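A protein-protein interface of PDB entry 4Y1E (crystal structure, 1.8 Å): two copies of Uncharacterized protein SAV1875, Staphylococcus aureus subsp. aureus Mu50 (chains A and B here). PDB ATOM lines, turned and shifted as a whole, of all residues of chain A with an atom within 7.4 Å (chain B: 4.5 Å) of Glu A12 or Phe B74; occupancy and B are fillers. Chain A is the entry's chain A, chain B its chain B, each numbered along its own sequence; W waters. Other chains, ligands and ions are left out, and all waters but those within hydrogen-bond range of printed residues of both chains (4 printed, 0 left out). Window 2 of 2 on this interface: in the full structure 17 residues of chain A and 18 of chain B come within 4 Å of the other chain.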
ATOM      1  N   LEU A   9     -26.464 -28.636  26.862  1.00  0.00           N
ATOM      2  CA  LEU A   9     -27.479 -28.414  25.837  1.00  0.00           C
ATOM      3  C   LEU A   9     -28.201 -27.069  26.066  1.00  0.00           C
ATOM      4  O   LEU A   9     -28.597 -26.727  27.206  1.00  0.00           O
ATOM      5  CB  LEU A   9     -28.525 -29.542  25.906  1.00  0.00           C
ATOM      6  CG  LEU A   9     -28.677 -30.612  24.828  1.00  0.00           C
ATOM      7  CD1 LEU A   9     -30.112 -31.088  24.710  1.00  0.00           C
ATOM      8  CD2 LEU A   9     -28.002 -30.360  23.485  1.00  0.00           C
ATOM      9  N   ALA A  10     -28.301 -26.281  25.000  1.00  0.00           N
ATOM     10  CA  ALA A  10     -29.220 -25.139  24.926  1.00  0.00           C
ATOM     11  C   ALA A  10     -30.211 -25.387  23.784  1.00  0.00           C
ATOM     12  O   ALA A  10     -30.153 -26.422  23.128  1.00  0.00           O
ATOM     13  CB  ALA A  10     -28.430 -23.853  24.669  1.00  0.00           C
ATOM     14  N   ASN A  11     -31.139 -24.455  23.576  1.00  0.00           N
ATOM     15  CA  ASN A  11     -31.997 -24.513  22.397  1.00  0.00           C
ATOM     16  C   ASN A  11     -31.262 -24.607  21.063  1.00  0.00           C
ATOM     17  O   ASN A  11     -30.125 -24.120  20.925  1.00  0.00           O
ATOM     18  CB  ASN A  11     -32.966 -23.331  22.407  1.00  0.00           C
ATOM     19  CG  ASN A  11     -33.986 -23.440  23.519  1.00  0.00           C
ATOM     20  OD1 ASN A  11     -34.774 -24.378  23.548  1.00  0.00           O
ATOM     21  ND2 ASN A  11     -33.921 -22.528  24.486  1.00  0.00           N
ATOM     22  N   GLU A  12     -31.945 -25.181  20.072  1.00  0.00           N
ATOM     23  CA  GLU A  12     -31.494 -25.220  18.679  1.00  0.00           C
ATOM     24  C   GLU A  12     -30.219 -26.042  18.509  1.00  0.00           C
ATOM     25  O   GLU A  12     -29.460 -25.852  17.542  1.00  0.00           O
ATOM     26  CB  GLU A  12     -31.293 -23.798  18.127  1.00  0.00           C
ATOM     27  CG  GLU A  12     -32.552 -22.958  18.257  1.00  0.00           C
ATOM     28  CD  GLU A  12     -32.411 -21.612  17.599  1.00  0.00           C
ATOM     29  OE1 GLU A  12     -31.854 -20.713  18.237  1.00  0.00           O
ATOM     30  OE2 GLU A  12     -32.794 -21.476  16.421  1.00  0.00           O
ATOM     31  N   PHE A  13     -30.089 -27.067  19.339  1.00  0.00           N
ATOM     32  CA  PHE A  13     -29.182 -28.149  19.062  1.00  0.00           C
ATOM     33  C   PHE A  13     -29.619 -28.962  17.835  1.00  0.00           C
ATOM     34  O   PHE A  13     -30.804 -28.953  17.415  1.00  0.00           O
ATOM     35  CB  PHE A  13     -29.040 -29.055  20.311  1.00  0.00           C
ATOM     36  CG  PHE A  13     -30.320 -29.750  20.720  1.00  0.00           C
ATOM     37  CD1 PHE A  13     -31.214 -29.127  21.583  1.00  0.00           C
ATOM     38  CD2 PHE A  13     -30.607 -31.032  20.274  1.00  0.00           C
ATOM     39  CE1 PHE A  13     -32.378 -29.756  21.974  1.00  0.00           C
ATOM     40  CE2 PHE A  13     -31.742 -31.694  20.705  1.00  0.00           C
ATOM     41  CZ  PHE A  13     -32.608 -31.065  21.580  1.00  0.00           C
ATOM     42  N   GLU A  14     -28.634 -29.551  17.169  1.00  0.00           N
ATOM     43  CA  GLU A  14     -28.924 -30.460  16.059  1.00  0.00           C
ATOM     44  C   GLU A  14     -29.466 -31.769  16.641  1.00  0.00           C
ATOM     45  O   GLU A  14     -28.766 -32.484  17.370  1.00  0.00           O
ATOM     46  CB  GLU A  14     -27.668 -30.742  15.230  1.00  0.00           C
ATOM     47  CG  GLU A  14     -27.940 -31.721  14.093  1.00  0.00           C
ATOM     48  CD  GLU A  14     -28.679 -31.050  12.958  1.00  0.00           C
ATOM     49  OE1 GLU A  14     -28.178 -30.021  12.489  1.00  0.00           O
ATOM     50  OE2 GLU A  14     -29.788 -31.495  12.592  1.00  0.00           O
ATOM     51  N   ASP A  15     -30.769 -31.964  16.468  1.00  0.00           N
ATOM     52  CA  ASP A  15     -31.513 -33.010  17.186  1.00  0.00           C
ATOM     53  C   ASP A  15     -30.752 -34.347  17.231  1.00  0.00           C
ATOM     54  O   ASP A  15     -30.625 -34.978  18.291  1.00  0.00           O
ATOM     55  CB  ASP A  15     -32.886 -33.237  16.526  1.00  0.00           C
ATOM     56  CG  ASP A  15     -33.752 -31.980  16.478  1.00  0.00           C
ATOM     57  OD1 ASP A  15     -33.215 -30.868  16.311  1.00  0.00           O
ATOM     58  OD2 ASP A  15     -34.995 -32.131  16.437  1.00  0.00           O
ATOM     59  N   VAL A  43     -35.427 -27.714  26.574  1.00  0.00           N
ATOM     60  CA  VAL A  43     -34.780 -27.127  25.403  1.00  0.00           C
ATOM     61  C   VAL A  43     -35.255 -27.853  24.160  1.00  0.00           C
ATOM     62  O   VAL A  43     -35.714 -28.987  24.245  1.00  0.00           O
ATOM     63  CB  VAL A  43     -33.241 -27.144  25.478  1.00  0.00           C
ATOM     64  CG1 VAL A  43     -32.735 -26.137  26.532  1.00  0.00           C
ATOM     65  CG2 VAL A  43     -32.736 -28.549  25.774  1.00  0.00           C
ATOM     66  N   VAL A  44     -35.311 -27.130  23.054  1.00  0.00           N
ATOM     67  CA  VAL A  44     -35.936 -27.651  21.825  1.00  0.00           C
ATOM     68  C   VAL A  44     -34.939 -27.618  20.667  1.00  0.00           C
ATOM     69  O   VAL A  44     -34.378 -26.557  20.333  1.00  0.00           O
ATOM     70  CB  VAL A  44     -37.170 -26.815  21.440  1.00  0.00           C
ATOM     71  CG1 VAL A  44     -37.828 -27.395  20.182  1.00  0.00           C
ATOM     72  CG2 VAL A  44     -38.157 -26.755  22.613  1.00  0.00           C
ATOM     73  N   GLY A  45     -34.748 -28.770  20.035  1.00  0.00           N
ATOM     74  CA  GLY A  45     -33.831 -28.901  18.908  1.00  0.00           C
ATOM     75  C   GLY A  45     -34.220 -28.053  17.708  1.00  0.00           C
ATOM     76  O   GLY A  45     -35.387 -27.694  17.539  1.00  0.00           O
ATOM     77  N   LYS A  46     -33.265 -27.858  16.806  1.00  0.00           N
ATOM     78  CA  LYS A  46     -33.507 -27.180  15.544  1.00  0.00           C
ATOM     79  C   LYS A  46     -34.684 -27.767  14.809  1.00  0.00           C
ATOM     80  O   LYS A  46     -35.205 -27.130  13.901  1.00  0.00           O
ATOM     81  CB  LYS A  46     -32.282 -27.313  14.639  1.00  0.00           C
ATOM     82  CG  LYS A  46     -31.151 -26.399  15.006  1.00  0.00           C
ATOM     83  CD  LYS A  46     -29.927 -26.797  14.206  1.00  0.00           C
ATOM     84  CE  LYS A  46     -29.765 -25.862  13.024  1.00  0.00           C
ATOM     85  NZ  LYS A  46     -30.625 -26.312  11.891  1.00  0.00           N
ATOM     86  N   HIS A  47     -34.898 -29.064  14.991  1.00  0.00           N
ATOM     87  CA  HIS A  47     -35.986 -29.764  14.278  1.00  0.00           C
ATOM     88  C   HIS A  47     -37.071 -30.239  15.202  1.00  0.00           C
ATOM     89  O   HIS A  47     -37.904 -31.074  14.826  1.00  0.00           O
ATOM     90  CB  HIS A  47     -35.433 -30.915  13.444  1.00  0.00           C
ATOM     91  CG  HIS A  47     -34.314 -30.500  12.516  1.00  0.00           C
ATOM     92  ND1 HIS A  47     -34.510 -29.652  11.480  1.00  0.00           N
ATOM     93  CD2 HIS A  47     -32.938 -30.725  12.584  1.00  0.00           C
ATOM     94  CE1 HIS A  47     -33.334 -29.408  10.870  1.00  0.00           C
ATOM     95  NE2 HIS A  47     -32.368 -30.064  11.549  1.00  0.00           N
ATOM     96  N   GLU A  49     -37.175 -31.558  18.448  1.00  0.00           N
ATOM     97  CA  GLU A  49     -37.039 -32.541  19.528  1.00  0.00           C
ATOM     98  C   GLU A  49     -37.059 -31.807  20.855  1.00  0.00           C
ATOM     99  O   GLU A  49     -36.299 -30.848  21.051  1.00  0.00           O
ATOM    100  CB  GLU A  49     -35.717 -33.299  19.406  1.00  0.00           C
ATOM    101  CG  GLU A  49     -35.442 -34.178  20.619  1.00  0.00           C
ATOM    102  CD  GLU A  49     -35.027 -35.581  20.239  1.00  0.00           C
ATOM    103  OE1 GLU A  49     -35.211 -35.957  19.062  1.00  0.00           O
ATOM    104  OE2 GLU A  49     -34.524 -36.312  21.120  1.00  0.00           O
ATOM    105  N   PRO A  71     -23.289 -31.685  21.838  1.00  0.00           N
ATOM    106  CA  PRO A  71     -23.929 -31.747  20.525  1.00  0.00           C
ATOM    107  C   PRO A  71     -23.808 -30.417  19.787  1.00  0.00           C
ATOM    108  O   PRO A  71     -23.664 -29.382  20.440  1.00  0.00           O
ATOM    109  CB  PRO A  71     -25.407 -32.009  20.876  1.00  0.00           C
ATOM    110  CG  PRO A  71     -25.328 -32.766  22.200  1.00  0.00           C
ATOM    111  CD  PRO A  71     -24.223 -32.026  22.930  1.00  0.00           C
ATOM    112  N   GLY A  72     -23.913 -30.447  18.455  1.00  0.00           N
ATOM    113  CA  GLY A  72     -23.726 -29.221  17.671  1.00  0.00           C
ATOM    114  C   GLY A  72     -25.055 -28.540  17.359  1.00  0.00           C
ATOM    115  O   GLY A  72     -25.843 -28.241  18.263  1.00  0.00           O
ATOM    116  N   GLY A  73     -25.210 -28.117  16.113  1.00  0.00           N
ATOM    117  CA  GLY A  73     -26.206 -27.108  15.780  1.00  0.00           C
ATOM    118  C   GLY A  73     -25.835 -25.737  16.346  1.00  0.00           C
ATOM    119  O   GLY A  73     -24.658 -25.383  16.418  1.00  0.00           O
ATOM    120  N   PHE A  74     -26.837 -24.960  16.744  1.00  0.00           N
ATOM    121  CA  PHE A  74     -26.585 -23.640  17.321  1.00  0.00           C
ATOM    122  C   PHE A  74     -26.611 -23.644  18.848  1.00  0.00           C
ATOM    123  O   PHE A  74     -26.480 -22.581  19.468  1.00  0.00           O
ATOM    124  CB  PHE A  74     -27.585 -22.625  16.777  1.00  0.00           C
ATOM    125  CG  PHE A  74     -27.476 -22.431  15.295  1.00  0.00           C
ATOM    126  CD1 PHE A  74     -26.236 -22.240  14.704  1.00  0.00           C
ATOM    127  CD2 PHE A  74     -28.593 -22.559  14.491  1.00  0.00           C
ATOM    128  CE1 PHE A  74     -26.113 -22.171  13.318  1.00  0.00           C
ATOM    129  CE2 PHE A  74     -28.489 -22.429  13.106  1.00  0.00           C
ATOM    130  CZ  PHE A  74     -27.248 -22.239  12.523  1.00  0.00           C
ATOM    131  N   SER A  75     -26.725 -24.838  19.441  1.00  0.00           N
ATOM    132  CA  SER A  75     -26.685 -24.973  20.912  1.00  0.00           C
ATOM    133  C   SER A  75     -25.379 -24.455  21.499  1.00  0.00           C
ATOM    134  O   SER A  75     -25.407 -23.617  22.394  1.00  0.00           O
ATOM    135  CB  SER A  75     -26.972 -26.418  21.375  1.00  0.00           C
ATOM    136  OG  SER A  75     -26.607 -26.612  22.756  1.00  0.00           O
ATOM    137  N   PRO A  76     -24.235 -24.842  20.903  1.00  0.00           N
ATOM    138  CA  PRO A  76     -22.992 -24.311  21.464  1.00  0.00           C
ATOM    139  C   PRO A  76     -22.900 -22.775  21.449  1.00  0.00           C
ATOM    140  O   PRO A  76     -22.482 -22.145  22.443  1.00  0.00           O
ATOM    141  CB  PRO A  76     -21.909 -24.942  20.575  1.00  0.00           C
ATOM    142  CG  PRO A  76     -22.515 -26.258  20.150  1.00  0.00           C
ATOM    143  CD  PRO A  76     -23.999 -25.947  19.956  1.00  0.00           C
ATOM    144  N   ASP A  77     -23.245 -22.173  20.322  1.00  0.00           N
ATOM    145  CA  ASP A  77     -23.310 -20.721  20.248  1.00  0.00           C
ATOM    146  C   ASP A  77     -24.165 -20.107  21.365  1.00  0.00           C
ATOM    147  O   ASP A  77     -23.716 -19.173  22.030  1.00  0.00           O
ATOM    148  CB  ASP A  77     -23.823 -20.271  18.874  1.00  0.00           C
ATOM    149  CG  ASP A  77     -23.641 -18.769  18.662  1.00  0.00           C
ATOM    150  OD1 ASP A  77     -22.524 -18.368  18.300  1.00  0.00           O
ATOM    151  OD2 ASP A  77     -24.546 -18.009  19.044  1.00  0.00           O
ATOM    152  N   HIS A  78     -25.371 -20.648  21.614  1.00  0.00           N
ATOM    153  CA  HIS A  78     -26.156 -20.202  22.763  1.00  0.00           C
ATOM    154  C   HIS A  78     -25.452 -20.323  24.090  1.00  0.00           C
ATOM    155  O   HIS A  78     -25.548 -19.425  24.960  1.00  0.00           O
ATOM    156  CB  HIS A  78     -27.511 -20.911  22.805  1.00  0.00           C
ATOM    157  CG  HIS A  78     -28.476 -20.441  21.741  1.00  0.00           C
ATOM    158  ND1 HIS A  78     -28.840 -19.141  21.599  1.00  0.00           N
ATOM    159  CD2 HIS A  78     -29.138 -21.146  20.733  1.00  0.00           C
ATOM    160  CE1 HIS A  78     -29.750 -19.040  20.600  1.00  0.00           C
ATOM    161  NE2 HIS A  78     -29.973 -20.286  20.111  1.00  0.00           N
ATOM    162  N   ASN A 127     -17.593 -24.703   9.275  1.00  0.00           N
ATOM    163  CA  ASN A 127     -17.944 -23.334   9.720  1.00  0.00           C
ATOM    164  C   ASN A 127     -17.052 -22.786  10.840  1.00  0.00           C
ATOM    165  O   ASN A 127     -16.997 -21.597  11.031  1.00  0.00           O
ATOM    166  CB  ASN A 127     -19.391 -23.243  10.196  1.00  0.00           C
ATOM    167  CG  ASN A 127     -20.390 -23.855   9.219  1.00  0.00           C
ATOM    168  OD1 ASN A 127     -21.508 -23.342   9.083  1.00  0.00           O
ATOM    169  ND2 ASN A 127     -20.042 -24.988   8.613  1.00  0.00           N
ATOM    170  N   ASN B  11     -29.803 -17.829   4.982  1.00  0.00           N
ATOM    171  CA  ASN B  11     -30.971 -18.051   5.813  1.00  0.00           C
ATOM    172  C   ASN B  11     -30.664 -17.804   7.303  1.00  0.00           C
ATOM    173  O   ASN B  11     -29.508 -17.921   7.729  1.00  0.00           O
ATOM    174  CB  ASN B  11     -31.486 -19.481   5.610  1.00  0.00           C
ATOM    175  CG  ASN B  11     -32.194 -19.652   4.277  1.00  0.00           C
ATOM    176  OD1 ASN B  11     -33.175 -18.970   3.992  1.00  0.00           O
ATOM    177  ND2 ASN B  11     -31.670 -20.535   3.436  1.00  0.00           N
ATOM    178  N   GLU B  12     -31.706 -17.457   8.064  1.00  0.00           N
ATOM    179  CA  GLU B  12     -31.661 -17.304   9.529  1.00  0.00           C
ATOM    180  C   GLU B  12     -30.863 -16.080  10.000  1.00  0.00           C
ATOM    181  O   GLU B  12     -30.396 -16.023  11.162  1.00  0.00           O
ATOM    182  CB  GLU B  12     -31.159 -18.577  10.224  1.00  0.00           C
ATOM    183  CG  GLU B  12     -31.942 -19.821   9.814  1.00  0.00           C
ATOM    184  CD  GLU B  12     -31.525 -21.058  10.596  1.00  0.00           C
ATOM    185  OE1 GLU B  12     -30.571 -21.744  10.168  1.00  0.00           O
ATOM    186  OE2 GLU B  12     -32.007 -21.226  11.725  1.00  0.00           O
ATOM    187  N   LYS B  46     -34.584 -15.390  10.647  1.00  0.00           N
ATOM    188  CA  LYS B  46     -34.957 -16.274  11.740  1.00  0.00           C
ATOM    189  C   LYS B  46     -36.310 -15.925  12.343  1.00  0.00           C
ATOM    190  O   LYS B  46     -36.932 -16.766  13.000  1.00  0.00           O
ATOM    191  CB  LYS B  46     -33.848 -16.380  12.799  1.00  0.00           C
ATOM    192  CG  LYS B  46     -33.621 -15.121  13.594  1.00  0.00           C
ATOM    193  CD  LYS B  46     -32.210 -15.103  14.175  1.00  0.00           C
ATOM    194  CE  LYS B  46     -32.022 -16.261  15.135  1.00  0.00           C
ATOM    195  NZ  LYS B  46     -33.014 -16.249  16.247  1.00  0.00           N
ATOM    196  N   GLY B  72     -26.402 -10.114  11.325  1.00  0.00           N
ATOM    197  CA  GLY B  72     -26.096 -11.232  12.236  1.00  0.00           C
ATOM    198  C   GLY B  72     -27.201 -12.280  12.269  1.00  0.00           C
ATOM    199  O   GLY B  72     -27.695 -12.705  11.220  1.00  0.00           O
ATOM    200  N   GLY B  73     -27.549 -12.727  13.472  1.00  0.00           N
ATOM    201  CA  GLY B  73     -28.242 -13.999  13.639  1.00  0.00           C
ATOM    202  C   GLY B  73     -27.326 -15.125  13.203  1.00  0.00           C
ATOM    203  O   GLY B  73     -26.128 -15.099  13.472  1.00  0.00           O
ATOM    204  N   PHE B  74     -27.905 -16.176  12.652  1.00  0.00           N
ATOM    205  CA  PHE B  74     -27.103 -17.323  12.228  1.00  0.00           C
ATOM    206  C   PHE B  74     -26.746 -17.265  10.734  1.00  0.00           C
ATOM    207  O   PHE B  74     -26.198 -18.226  10.172  1.00  0.00           O
ATOM    208  CB  PHE B  74     -27.837 -18.605  12.595  1.00  0.00           C
ATOM    209  CG  PHE B  74     -28.014 -18.792  14.090  1.00  0.00           C
ATOM    210  CD1 PHE B  74     -26.931 -18.607  14.950  1.00  0.00           C
ATOM    211  CD2 PHE B  74     -29.264 -19.019  14.638  1.00  0.00           C
ATOM    212  CE1 PHE B  74     -27.086 -18.734  16.328  1.00  0.00           C
ATOM    213  CE2 PHE B  74     -29.418 -19.193  16.015  1.00  0.00           C
ATOM    214  CZ  PHE B  74     -28.338 -19.009  16.851  1.00  0.00           C
ATOM    215  N   SER B  75     -27.011 -16.124  10.087  1.00  0.00           N
ATOM    216  CA  SER B  75     -26.606 -15.987   8.678  1.00  0.00           C
ATOM    217  C   SER B  75     -25.081 -16.119   8.495  1.00  0.00           C
ATOM    218  O   SER B  75     -24.605 -16.928   7.659  1.00  0.00           O
ATOM    219  CB  SER B  75     -27.130 -14.672   8.076  1.00  0.00           C
ATOM    220  OG  SER B  75     -26.543 -14.456   6.802  1.00  0.00           O
ATOM    221  N   PRO B  76     -24.303 -15.391   9.315  1.00  0.00           N
ATOM    222  CA  PRO B  76     -22.859 -15.478   9.162  1.00  0.00           C
ATOM    223  C   PRO B  76     -22.355 -16.912   9.318  1.00  0.00           C
ATOM    224  O   PRO B  76     -21.540 -17.388   8.520  1.00  0.00           O
ATOM    225  CB  PRO B  76     -22.335 -14.549  10.272  1.00  0.00           C
ATOM    226  CG  PRO B  76     -23.410 -13.508  10.382  1.00  0.00           C
ATOM    227  CD  PRO B  76     -24.689 -14.309  10.238  1.00  0.00           C
ATOM    228  N   ASP B  77     -22.975 -17.672  10.210  1.00  0.00           N
ATOM    229  CA  ASP B  77     -22.559 -19.065  10.376  1.00  0.00           C
ATOM    230  C   ASP B  77     -22.756 -19.892   9.122  1.00  0.00           C
ATOM    231  O   ASP B  77     -21.875 -20.648   8.750  1.00  0.00           O
ATOM    232  CB  ASP B  77     -23.225 -19.754  11.573  1.00  0.00           C
ATOM    233  CG  ASP B  77     -22.606 -21.127  11.856  1.00  0.00           C
ATOM    234  OD1 ASP B  77     -21.537 -21.185  12.476  1.00  0.00           O
ATOM    235  OD2 ASP B  77     -23.138 -22.128  11.361  1.00  0.00           O
ATOM    236  N   HIS B  78     -23.928 -19.775   8.504  1.00  0.00           N
ATOM    237  CA  HIS B  78     -24.174 -20.407   7.223  1.00  0.00           C
ATOM    238  C   HIS B  78     -23.205 -20.004   6.154  1.00  0.00           C
ATOM    239  O   HIS B  78     -22.766 -20.856   5.382  1.00  0.00           O
ATOM    240  CB  HIS B  78     -25.596 -20.164   6.759  1.00  0.00           C
ATOM    241  CG  HIS B  78     -26.635 -20.838   7.611  1.00  0.00           C
ATOM    242  ND1 HIS B  78     -26.562 -22.147   7.949  1.00  0.00           N
ATOM    243  CD2 HIS B  78     -27.764 -20.326   8.255  1.00  0.00           C
ATOM    244  CE1 HIS B  78     -27.655 -22.480   8.671  1.00  0.00           C
ATOM    245  NE2 HIS B  78     -28.388 -21.362   8.859  1.00  0.00           N
ATOM    246  N   HIS B 106     -23.524 -11.331  15.250  1.00  0.00           N
ATOM    247  CA  HIS B 106     -22.619 -12.387  14.769  1.00  0.00           C
ATOM    248  C   HIS B 106     -21.913 -12.038  13.480  1.00  0.00           C
ATOM    249  O   HIS B 106     -21.058 -12.793  13.024  1.00  0.00           O
ATOM    250  CB  HIS B 106     -23.377 -13.703  14.533  1.00  0.00           C
ATOM    251  CG  HIS B 106     -23.827 -14.388  15.793  1.00  0.00           C
ATOM    252  ND1 HIS B 106     -24.937 -14.006  16.472  1.00  0.00           N
ATOM    253  CD2 HIS B 106     -23.390 -15.562  16.389  1.00  0.00           C
ATOM    254  CE1 HIS B 106     -25.209 -14.929  17.419  1.00  0.00           C
ATOM    255  NE2 HIS B 106     -24.180 -15.776  17.469  1.00  0.00           N
HETATM  256  O   HOH W   1     -32.107 -17.936  18.176  1.00  0.00           O
HETATM  257  O   HOH W   2     -30.015 -24.293  10.151  1.00  0.00           O
HETATM  258  O   HOH W   3     -33.183 -19.330  14.975  1.00  0.00           O
HETATM  259  O   HOH W   4     -19.262 -19.802  12.329  1.00  0.00           O
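A ring nitrogen (NE2) of His B106 is in hydrogen-bond range of the side-chain carboxylate (OD2) of Asp A77, 2.8 Å away. OD1 of Asn A127 lies close to O of Asp B77, at 2.7 Å.
The side-chain carboxylate of Glu B12 sits at hydrogen-bond distance from a ring nitrogen (NE2) of His B78 (2.6 Å). N of Glu A12 is in hydrogen-bond range of O of Val A44 (2.8 Å). The backbone NH (N) of Phe B74 is in hydrogen-bond range of the backbone carbonyl oxygen (O) of Glu B12 (2.9 Å). A ring nitrogen (ND1) of His B106 lies close to the backbone carbonyl oxygen of Gly B73 (3.4 Å). N of Phe A74 lies within hydrogen-bond range of O of Glu A12, 2.9 Å away. The backbone carbonyl oxygen (O) of Glu A12 lies within hydrogen-bond range of the backbone NH (N) of Ser A75, at 3.5 Å.
Among the printed residues, merely in contact across the chains: Glu A12 with Phe B74 (3.6 Å), Phe A74 with Glu B12 (3.7 Å), Phe A74 with Phe B74 (3.6 Å), Phe A74 with Asp B77 (3.6 Å), Phe A74 with His B78 (3.9 Å), Asp A77 with Phe B74 (3.8 Å) and His A78 with Phe B74 (3.9 Å).
Of the printed residues of chain B, Glu A12 touches Phe B74 (3.6 Å). Lys A46 touches none of the printed residues of chain B. Ser A75 touches none of the printed residues of chain B. Phe B74 touches just these residues of chain A: Glu A12 (3.6 Å), Phe A74 (3.6 Å), Asp A77 (3.8 Å) and His A78 (3.9 Å). Of the printed residues of chain A, His B78 touches Phe A74. Printed residues of chain A within 4 Å of His B106: Asp A77. The nearest printed residue of chain B that does not touch Glu A12 is Glu B12 (4.8 Å). The nearest printed residue of chain A that does not touch Glu B12 is Glu A12 (4.8 Å).
Printed residues of chain A that touch a printed residue of chain B: Glu A12, Phe A74, Asp A77, His A78 and Asn A127. Of the 11 printed residues of chain B, 5 touch a printed residue of chain A. Printed residues of chain B that touch a printed residue of chain A: Glu B12, Phe B74, Asp B77, His B78 and His B106. Hydrophobic or aromatic side chains of chain B that line the printed part of chain A: Phe B74, His B78 and His B106.
Glu A12 touches Phe B74, and with the chains exchanged Phe A74 touches Glu B12. Phe B74 touches its own counterpart, Phe A74. Phe A74 touches Asp B77, and with the chains exchanged Asp A77 touches Phe B74. Phe A74 touches His B78, and with the chains exchanged His A78 touches Phe B74.
Water W2 bridges the side-chain carboxylate (OE1) of Glu B12 (2.6 Å) and the side-chain amino group (NZ) of Lys A46 (2.7 Å). Water W3 bridges OE2 of Glu A12 and NZ of Lys B46. Water W4 lies within hydrogen-bond range of OD1 of Asp B77 (2.7 Å) and O of Asn A127 (3.2 Å). Water W1 lies within hydrogen-bond range of NZ of Lys B46 (2.7 Å) and OE1 of Glu A12 (2.8 Å).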
